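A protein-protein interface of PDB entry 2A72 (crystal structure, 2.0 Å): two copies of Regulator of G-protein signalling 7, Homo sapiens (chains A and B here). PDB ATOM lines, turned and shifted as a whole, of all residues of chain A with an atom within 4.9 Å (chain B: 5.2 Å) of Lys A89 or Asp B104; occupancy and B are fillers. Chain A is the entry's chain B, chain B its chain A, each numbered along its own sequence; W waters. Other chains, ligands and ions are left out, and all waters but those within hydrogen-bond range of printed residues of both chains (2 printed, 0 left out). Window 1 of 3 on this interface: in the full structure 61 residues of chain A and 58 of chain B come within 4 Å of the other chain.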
ATOM      1  N   LYS A  85     -35.370  22.257  -2.787  1.00  0.00           N
ATOM      2  CA  LYS A  85     -33.955  21.881  -2.687  1.00  0.00           C
ATOM      3  C   LYS A  85     -33.060  22.873  -3.437  1.00  0.00           C
ATOM      4  O   LYS A  85     -32.111  23.431  -2.867  1.00  0.00           O
ATOM      5  CB  LYS A  85     -33.749  20.446  -3.197  1.00  0.00           C
ATOM      6  CG  LYS A  85     -32.343  19.902  -3.013  1.00  0.00           C
ATOM      7  N   SER A  86     -33.404  23.138  -4.695  1.00  0.00           N
ATOM      8  CA  SER A  86     -32.603  24.026  -5.523  1.00  0.00           C
ATOM      9  C   SER A  86     -32.738  25.500  -5.081  1.00  0.00           C
ATOM     10  O   SER A  86     -31.755  26.231  -5.156  1.00  0.00           O
ATOM     11  CB  SER A  86     -32.922  23.830  -7.013  1.00  0.00           C
ATOM     12  OG  SER A  86     -33.960  24.679  -7.448  1.00  0.00           O
ATOM     13  N   TYR A  87     -33.930  25.922  -4.624  1.00  0.00           N
ATOM     14  CA  TYR A  87     -34.125  27.261  -4.018  1.00  0.00           C
ATOM     15  C   TYR A  87     -33.179  27.415  -2.805  1.00  0.00           C
ATOM     16  O   TYR A  87     -32.425  28.381  -2.729  1.00  0.00           O
ATOM     17  CB  TYR A  87     -35.602  27.561  -3.594  1.00  0.00           C
ATOM     18  CG  TYR A  87     -36.122  28.944  -4.037  1.00  0.00           C
ATOM     19  CD1 TYR A  87     -35.490  30.123  -3.640  1.00  0.00           C
ATOM     20  CD2 TYR A  87     -37.240  29.062  -4.864  1.00  0.00           C
ATOM     21  CE1 TYR A  87     -35.938  31.389  -4.065  1.00  0.00           C
ATOM     22  CE2 TYR A  87     -37.709  30.321  -5.304  1.00  0.00           C
ATOM     23  CZ  TYR A  87     -37.055  31.491  -4.900  1.00  0.00           C
ATOM     24  OH  TYR A  87     -37.525  32.737  -5.347  1.00  0.00           O
ATOM     25  N   ASP A  88     -33.191  26.436  -1.908  1.00  0.00           N
ATOM     26  CA  ASP A  88     -32.366  26.493  -0.695  1.00  0.00           C
ATOM     27  C   ASP A  88     -30.887  26.665  -0.996  1.00  0.00           C
ATOM     28  O   ASP A  88     -30.235  27.561  -0.436  1.00  0.00           O
ATOM     29  CB  ASP A  88     -32.585  25.252   0.168  1.00  0.00           C
ATOM     30  CG  ASP A  88     -33.974  25.198   0.751  1.00  0.00           C
ATOM     31  OD1 ASP A  88     -34.638  26.253   0.725  1.00  0.00           O
ATOM     32  OD2 ASP A  88     -34.408  24.116   1.227  1.00  0.00           O
ATOM     33  N   LYS A  89     -30.373  25.845  -1.911  1.00  0.00           N
ATOM     34  CA  LYS A  89     -28.975  25.939  -2.298  1.00  0.00           C
ATOM     35  C   LYS A  89     -28.649  27.317  -2.833  1.00  0.00           C
ATOM     36  O   LYS A  89     -27.664  27.932  -2.429  1.00  0.00           O
ATOM     37  CB  LYS A  89     -28.621  24.893  -3.342  1.00  0.00           C
ATOM     38  CG  LYS A  89     -28.677  23.499  -2.828  1.00  0.00           C
ATOM     39  CD  LYS A  89     -27.918  22.545  -3.737  1.00  0.00           C
ATOM     40  CE  LYS A  89     -27.843  21.156  -3.126  1.00  0.00           C
ATOM     41  NZ  LYS A  89     -29.161  20.467  -3.115  1.00  0.00           N
ATOM     42  N   THR A  90     -29.508  27.797  -3.728  1.00  0.00           N
ATOM     43  CA  THR A  90     -29.323  29.073  -4.379  1.00  0.00           C
ATOM     44  C   THR A  90     -29.251  30.207  -3.380  1.00  0.00           C
ATOM     45  O   THR A  90     -28.332  31.003  -3.421  1.00  0.00           O
ATOM     46  CB  THR A  90     -30.464  29.345  -5.423  1.00  0.00           C
ATOM     47  OG1 THR A  90     -30.625  28.194  -6.262  1.00  0.00           O
ATOM     48  CG2 THR A  90     -30.142  30.556  -6.279  1.00  0.00           C
ATOM     49  N   THR A  91     -30.209  30.275  -2.472  1.00  0.00           N
ATOM     50  CA  THR A  91     -30.257  31.362  -1.470  1.00  0.00           C
ATOM     51  C   THR A  91     -28.983  31.384  -0.616  1.00  0.00           C
ATOM     52  O   THR A  91     -28.398  32.450  -0.400  1.00  0.00           O
ATOM     53  CB  THR A  91     -31.481  31.245  -0.546  1.00  0.00           C
ATOM     54  OG1 THR A  91     -31.308  30.136   0.348  1.00  0.00           O
ATOM     55  CG2 THR A  91     -32.766  31.056  -1.345  1.00  0.00           C
ATOM     56  N   HIS A  92     -28.547  30.199  -0.169  1.00  0.00           N
ATOM     57  CA  HIS A  92     -27.315  30.052   0.609  1.00  0.00           C
ATOM     58  C   HIS A  92     -26.119  30.542  -0.206  1.00  0.00           C
ATOM     59  O   HIS A  92     -25.270  31.271   0.310  1.00  0.00           O
ATOM     60  CB  HIS A  92     -27.094  28.583   1.050  1.00  0.00           C
ATOM     61  CG  HIS A  92     -27.934  28.160   2.219  1.00  0.00           C
ATOM     62  ND1 HIS A  92     -27.388  27.683   3.395  1.00  0.00           N
ATOM     63  CD2 HIS A  92     -29.282  28.120   2.394  1.00  0.00           C
ATOM     64  CE1 HIS A  92     -28.356  27.374   4.243  1.00  0.00           C
ATOM     65  NE2 HIS A  92     -29.516  27.632   3.663  1.00  0.00           N
ATOM     66  N   ASN A  93     -26.065  30.178  -1.486  1.00  0.00           N
ATOM     67  CA  ASN A  93     -24.998  30.663  -2.352  1.00  0.00           C
ATOM     68  C   ASN A  93     -24.968  32.178  -2.523  1.00  0.00           C
ATOM     69  O   ASN A  93     -23.890  32.762  -2.536  1.00  0.00           O
ATOM     70  CB  ASN A  93     -25.038  29.969  -3.720  1.00  0.00           C
ATOM     71  CG  ASN A  93     -24.644  28.491  -3.643  1.00  0.00           C
ATOM     72  OD1 ASN A  93     -23.987  28.043  -2.688  1.00  0.00           O
ATOM     73  ND2 ASN A  93     -25.047  27.725  -4.653  1.00  0.00           N
ATOM     74  N   GLU A 103     -20.278  21.752  -0.194  1.00  0.00           N
ATOM     75  CA  GLU A 103     -21.527  21.178   0.305  1.00  0.00           C
ATOM     76  C   GLU A 103     -21.781  19.747  -0.198  1.00  0.00           C
ATOM     77  O   GLU A 103     -22.089  18.858   0.602  1.00  0.00           O
ATOM     78  CB  GLU A 103     -22.728  22.080  -0.041  1.00  0.00           C
ATOM     79  CG  GLU A 103     -24.078  21.516   0.409  1.00  0.00           C
ATOM     80  CD  GLU A 103     -25.261  22.416   0.070  1.00  0.00           C
ATOM     81  OE1 GLU A 103     -25.056  23.603  -0.289  1.00  0.00           O
ATOM     82  OE2 GLU A 103     -26.411  21.927   0.137  1.00  0.00           O
ATOM     83  N   ASP A 104     -21.650  19.522  -1.500  1.00  0.00           N
ATOM     84  CA  ASP A 104     -21.875  18.185  -2.064  1.00  0.00           C
ATOM     85  C   ASP A 104     -20.751  17.216  -1.635  1.00  0.00           C
ATOM     86  O   ASP A 104     -21.020  16.066  -1.292  1.00  0.00           O
ATOM     87  CB  ASP A 104     -22.049  18.235  -3.583  1.00  0.00           C
ATOM     88  CG  ASP A 104     -23.397  18.861  -4.009  1.00  0.00           C
ATOM     89  OD1 ASP A 104     -23.844  19.843  -3.374  1.00  0.00           O
ATOM     90  OD2 ASP A 104     -24.017  18.378  -4.980  1.00  0.00           O
ATOM     91  N   LYS B  89     -17.996  19.650  -9.096  1.00  0.00           N
ATOM     92  CA  LYS B  89     -18.664  20.784  -8.479  1.00  0.00           C
ATOM     93  C   LYS B  89     -17.735  21.545  -7.545  1.00  0.00           C
ATOM     94  O   LYS B  89     -17.762  22.776  -7.506  1.00  0.00           O
ATOM     95  CB  LYS B  89     -19.874  20.329  -7.687  1.00  0.00           C
ATOM     96  CG  LYS B  89     -21.093  20.081  -8.490  1.00  0.00           C
ATOM     97  CD  LYS B  89     -22.291  19.880  -7.547  1.00  0.00           C
ATOM     98  CE  LYS B  89     -23.570  19.473  -8.280  1.00  0.00           C
ATOM     99  NZ  LYS B  89     -24.489  20.630  -8.583  1.00  0.00           N
ATOM    100  N   THR B 101     -23.147  29.657  -8.766  1.00  0.00           N
ATOM    101  CA  THR B 101     -24.203  29.929  -7.792  1.00  0.00           C
ATOM    102  C   THR B 101     -25.576  29.330  -8.167  1.00  0.00           C
ATOM    103  O   THR B 101     -26.296  28.841  -7.280  1.00  0.00           O
ATOM    104  CB  THR B 101     -24.391  31.441  -7.631  1.00  0.00           C
ATOM    105  OG1 THR B 101     -23.195  32.026  -7.095  1.00  0.00           O
ATOM    106  CG2 THR B 101     -25.582  31.758  -6.750  1.00  0.00           C
ATOM    107  N   PHE B 102     -25.915  29.381  -9.466  1.00  0.00           N
ATOM    108  CA  PHE B 102     -27.235  28.969  -9.983  1.00  0.00           C
ATOM    109  C   PHE B 102     -27.256  27.595 -10.665  1.00  0.00           C
ATOM    110  O   PHE B 102     -28.258  27.247 -11.301  1.00  0.00           O
ATOM    111  CB  PHE B 102     -27.816  30.043 -10.939  1.00  0.00           C
ATOM    112  CG  PHE B 102     -27.903  31.423 -10.310  1.00  0.00           C
ATOM    113  CD1 PHE B 102     -28.947  31.746  -9.442  1.00  0.00           C
ATOM    114  CD2 PHE B 102     -26.930  32.383 -10.570  1.00  0.00           C
ATOM    115  CE1 PHE B 102     -29.012  32.976  -8.852  1.00  0.00           C
ATOM    116  CE2 PHE B 102     -27.000  33.635  -9.991  1.00  0.00           C
ATOM    117  CZ  PHE B 102     -28.031  33.923  -9.102  1.00  0.00           C
ATOM    118  N   GLU B 103     -26.203  26.787 -10.477  1.00  0.00           N
ATOM    119  CA  GLU B 103     -26.069  25.495 -11.173  1.00  0.00           C
ATOM    120  C   GLU B 103     -27.284  24.565 -11.044  1.00  0.00           C
ATOM    121  O   GLU B 103     -27.827  24.092 -12.053  1.00  0.00           O
ATOM    122  CB  GLU B 103     -24.810  24.745 -10.703  1.00  0.00           C
ATOM    123  CG  GLU B 103     -24.533  23.423 -11.466  1.00  0.00           C
ATOM    124  CD  GLU B 103     -23.256  22.685 -10.987  1.00  0.00           C
ATOM    125  OE1 GLU B 103     -22.384  23.315 -10.313  1.00  0.00           O
ATOM    126  OE2 GLU B 103     -23.139  21.453 -11.263  1.00  0.00           O
ATOM    127  N   ASP B 104     -27.672  24.258  -9.810  1.00  0.00           N
ATOM    128  CA  ASP B 104     -28.808  23.369  -9.564  1.00  0.00           C
ATOM    129  C   ASP B 104     -30.163  23.973 -10.003  1.00  0.00           C
ATOM    130  O   ASP B 104     -31.028  23.264 -10.479  1.00  0.00           O
ATOM    131  CB  ASP B 104     -28.851  22.950  -8.092  1.00  0.00           C
ATOM    132  CG  ASP B 104     -27.720  21.958  -7.718  1.00  0.00           C
ATOM    133  OD1 ASP B 104     -26.642  21.963  -8.361  1.00  0.00           O
ATOM    134  OD2 ASP B 104     -27.912  21.172  -6.790  1.00  0.00           O
ATOM    135  N   ALA B 105     -30.329  25.282  -9.866  1.00  0.00           N
ATOM    136  CA  ALA B 105     -31.562  25.956 -10.296  1.00  0.00           C
ATOM    137  C   ALA B 105     -31.645  25.944 -11.818  1.00  0.00           C
ATOM    138  O   ALA B 105     -32.705  25.668 -12.373  1.00  0.00           O
ATOM    139  CB  ALA B 105     -31.590  27.392  -9.774  1.00  0.00           C
ATOM    140  N   GLN B 106     -30.526  26.243 -12.482  1.00  0.00           N
ATOM    141  CA  GLN B 106     -30.476  26.244 -13.928  1.00  0.00           C
ATOM    142  C   GLN B 106     -30.776  24.853 -14.485  1.00  0.00           C
ATOM    143  O   GLN B 106     -31.441  24.741 -15.495  1.00  0.00           O
ATOM    144  CB  GLN B 106     -29.128  26.729 -14.472  1.00  0.00           C
ATOM    145  CG  GLN B 106     -29.178  27.028 -16.014  1.00  0.00           C
ATOM    146  CD  GLN B 106     -27.818  27.281 -16.619  1.00  0.00           C
ATOM    147  OE1 GLN B 106     -26.808  26.845 -16.070  1.00  0.00           O
ATOM    148  NE2 GLN B 106     -27.782  27.974 -17.774  1.00  0.00           N
ATOM    149  N   GLU B 107     -30.290  23.807 -13.832  1.00  0.00           N
ATOM    150  CA  GLU B 107     -30.618  22.430 -14.276  1.00  0.00           C
ATOM    151  C   GLU B 107     -32.112  22.122 -14.123  1.00  0.00           C
ATOM    152  O   GLU B 107     -32.723  21.577 -15.056  1.00  0.00           O
ATOM    153  CB  GLU B 107     -29.765  21.386 -13.573  1.00  0.00           C
ATOM    154  CG  GLU B 107     -30.125  19.919 -13.885  1.00  0.00           C
ATOM    155  CD  GLU B 107     -29.892  19.427 -15.346  1.00  0.00           C
ATOM    156  OE1 GLU B 107     -29.684  20.219 -16.292  1.00  0.00           O
ATOM    157  OE2 GLU B 107     -29.949  18.185 -15.537  1.00  0.00           O
ATOM    158  N   HIS B 108     -32.692  22.510 -12.980  1.00  0.00           N
ATOM    159  CA  HIS B 108     -34.140  22.391 -12.765  1.00  0.00           C
ATOM    160  C   HIS B 108     -34.939  23.061 -13.889  1.00  0.00           C
ATOM    161  O   HIS B 108     -35.847  22.473 -14.461  1.00  0.00           O
ATOM    162  CB  HIS B 108     -34.536  23.032 -11.437  1.00  0.00           C
ATOM    163  CG  HIS B 108     -36.002  22.981 -11.158  1.00  0.00           C
ATOM    164  ND1 HIS B 108     -36.634  21.836 -10.734  1.00  0.00           N
ATOM    165  CD2 HIS B 108     -36.964  23.929 -11.259  1.00  0.00           C
ATOM    166  CE1 HIS B 108     -37.922  22.077 -10.576  1.00  0.00           C
ATOM    167  NE2 HIS B 108     -38.151  23.338 -10.895  1.00  0.00           N
HETATM  168  O   HOH W   1     -28.499  26.718  -7.786  1.00  0.00           O
HETATM  169  O   HOH W   2     -22.590  33.441  -4.791  1.00  0.00           O
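Water W2 lies within hydrogen-bond range of the backbone carbonyl oxygen (O) of Asn A93 (2.7 Å) and the side-chain hydroxyl (OG1) of Thr B101 (2.8 Å). Water W1 lies within hydrogen-bond range of the side-chain hydroxyl (OG1) of Thr A90, the backbone carbonyl oxygen (O) of Thr B101, the backbone NH (N) of Ala B105 and the backbone NH (N) of Asp B104.
Of the printed residues of chain B, Thr A90 touches Phe B102 (3.6 Å) and Ala B105 (3.7 Å). Of the printed residues of chain B, Asn A93 touches Thr B101 (3.1 Å). Of the printed residues of chain A, Lys B89 touches Asp A104. Printed residues of chain A within 4 Å of Phe B102: Thr A90 (3.6 Å). Printed residues of chain A within 4 Å of Asp B104: Ser A86 and Lys A89. Glu B107 touches none of the printed residues of chain A. The nearest printed residue of chain A that does not touch Asp B104 is Asp A104 (5.1 Å). The nearest printed residue of chain A that does not touch Thr B101 is Thr A90 (4.2 Å).
The side-chain amino group (NZ) of Lys B89 lies within salt-bridge range of the side-chain carboxylate (OE2) of Glu B103, 3.1 Å away. The side-chain carboxylate (OD1) of Asp B104 is in salt-bridge range of the side-chain amino group (NZ) of Lys B89, 2.5 Å away. OG1 of Thr A90 lies within hydrogen-bond range of O of Ser A86 (2.5 Å). ND2 of Asn A93 sits close to O of Lys A89, 3.4 Å away.
Lys A89 touches Asp B104, and with the chains exchanged Asp A104 touches Lys B89. Positions printed for both chains: 89, 103 and 104. Of the 7 pairs that touch across the chains among the printed residues, 2 have their exchanged pair printed and touching as well.
Of the 9 printed residues of chain B, 5 touch a printed residue of chain A. Hydrophobic or aromatic side chains of chain B that line the printed part of chain A: Phe B102 and Ala B105. Among the printed residues, 7 pairs touch across the chains.
The side-chain amide nitrogen (ND2) of Asn A93 is in hydrogen-bond range of the backbone carbonyl oxygen (O) of Thr B101 (3.1 Å). The side-chain amino group of Lys A89 lies within salt-bridge range of the side-chain carboxylate of Asp B104, 3.9 Å away.
Asp B104 touches Ser A86. Ser A86 touches Ala B105 (OG to CA, 3.9 Å). CG2 of Thr A90 touches CD1 of Phe B102, 3.6 Å away. Thr A90 touches Ala B105 (OG1 to CB, 3.7 Å). Asp A104 touches Lys B89.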
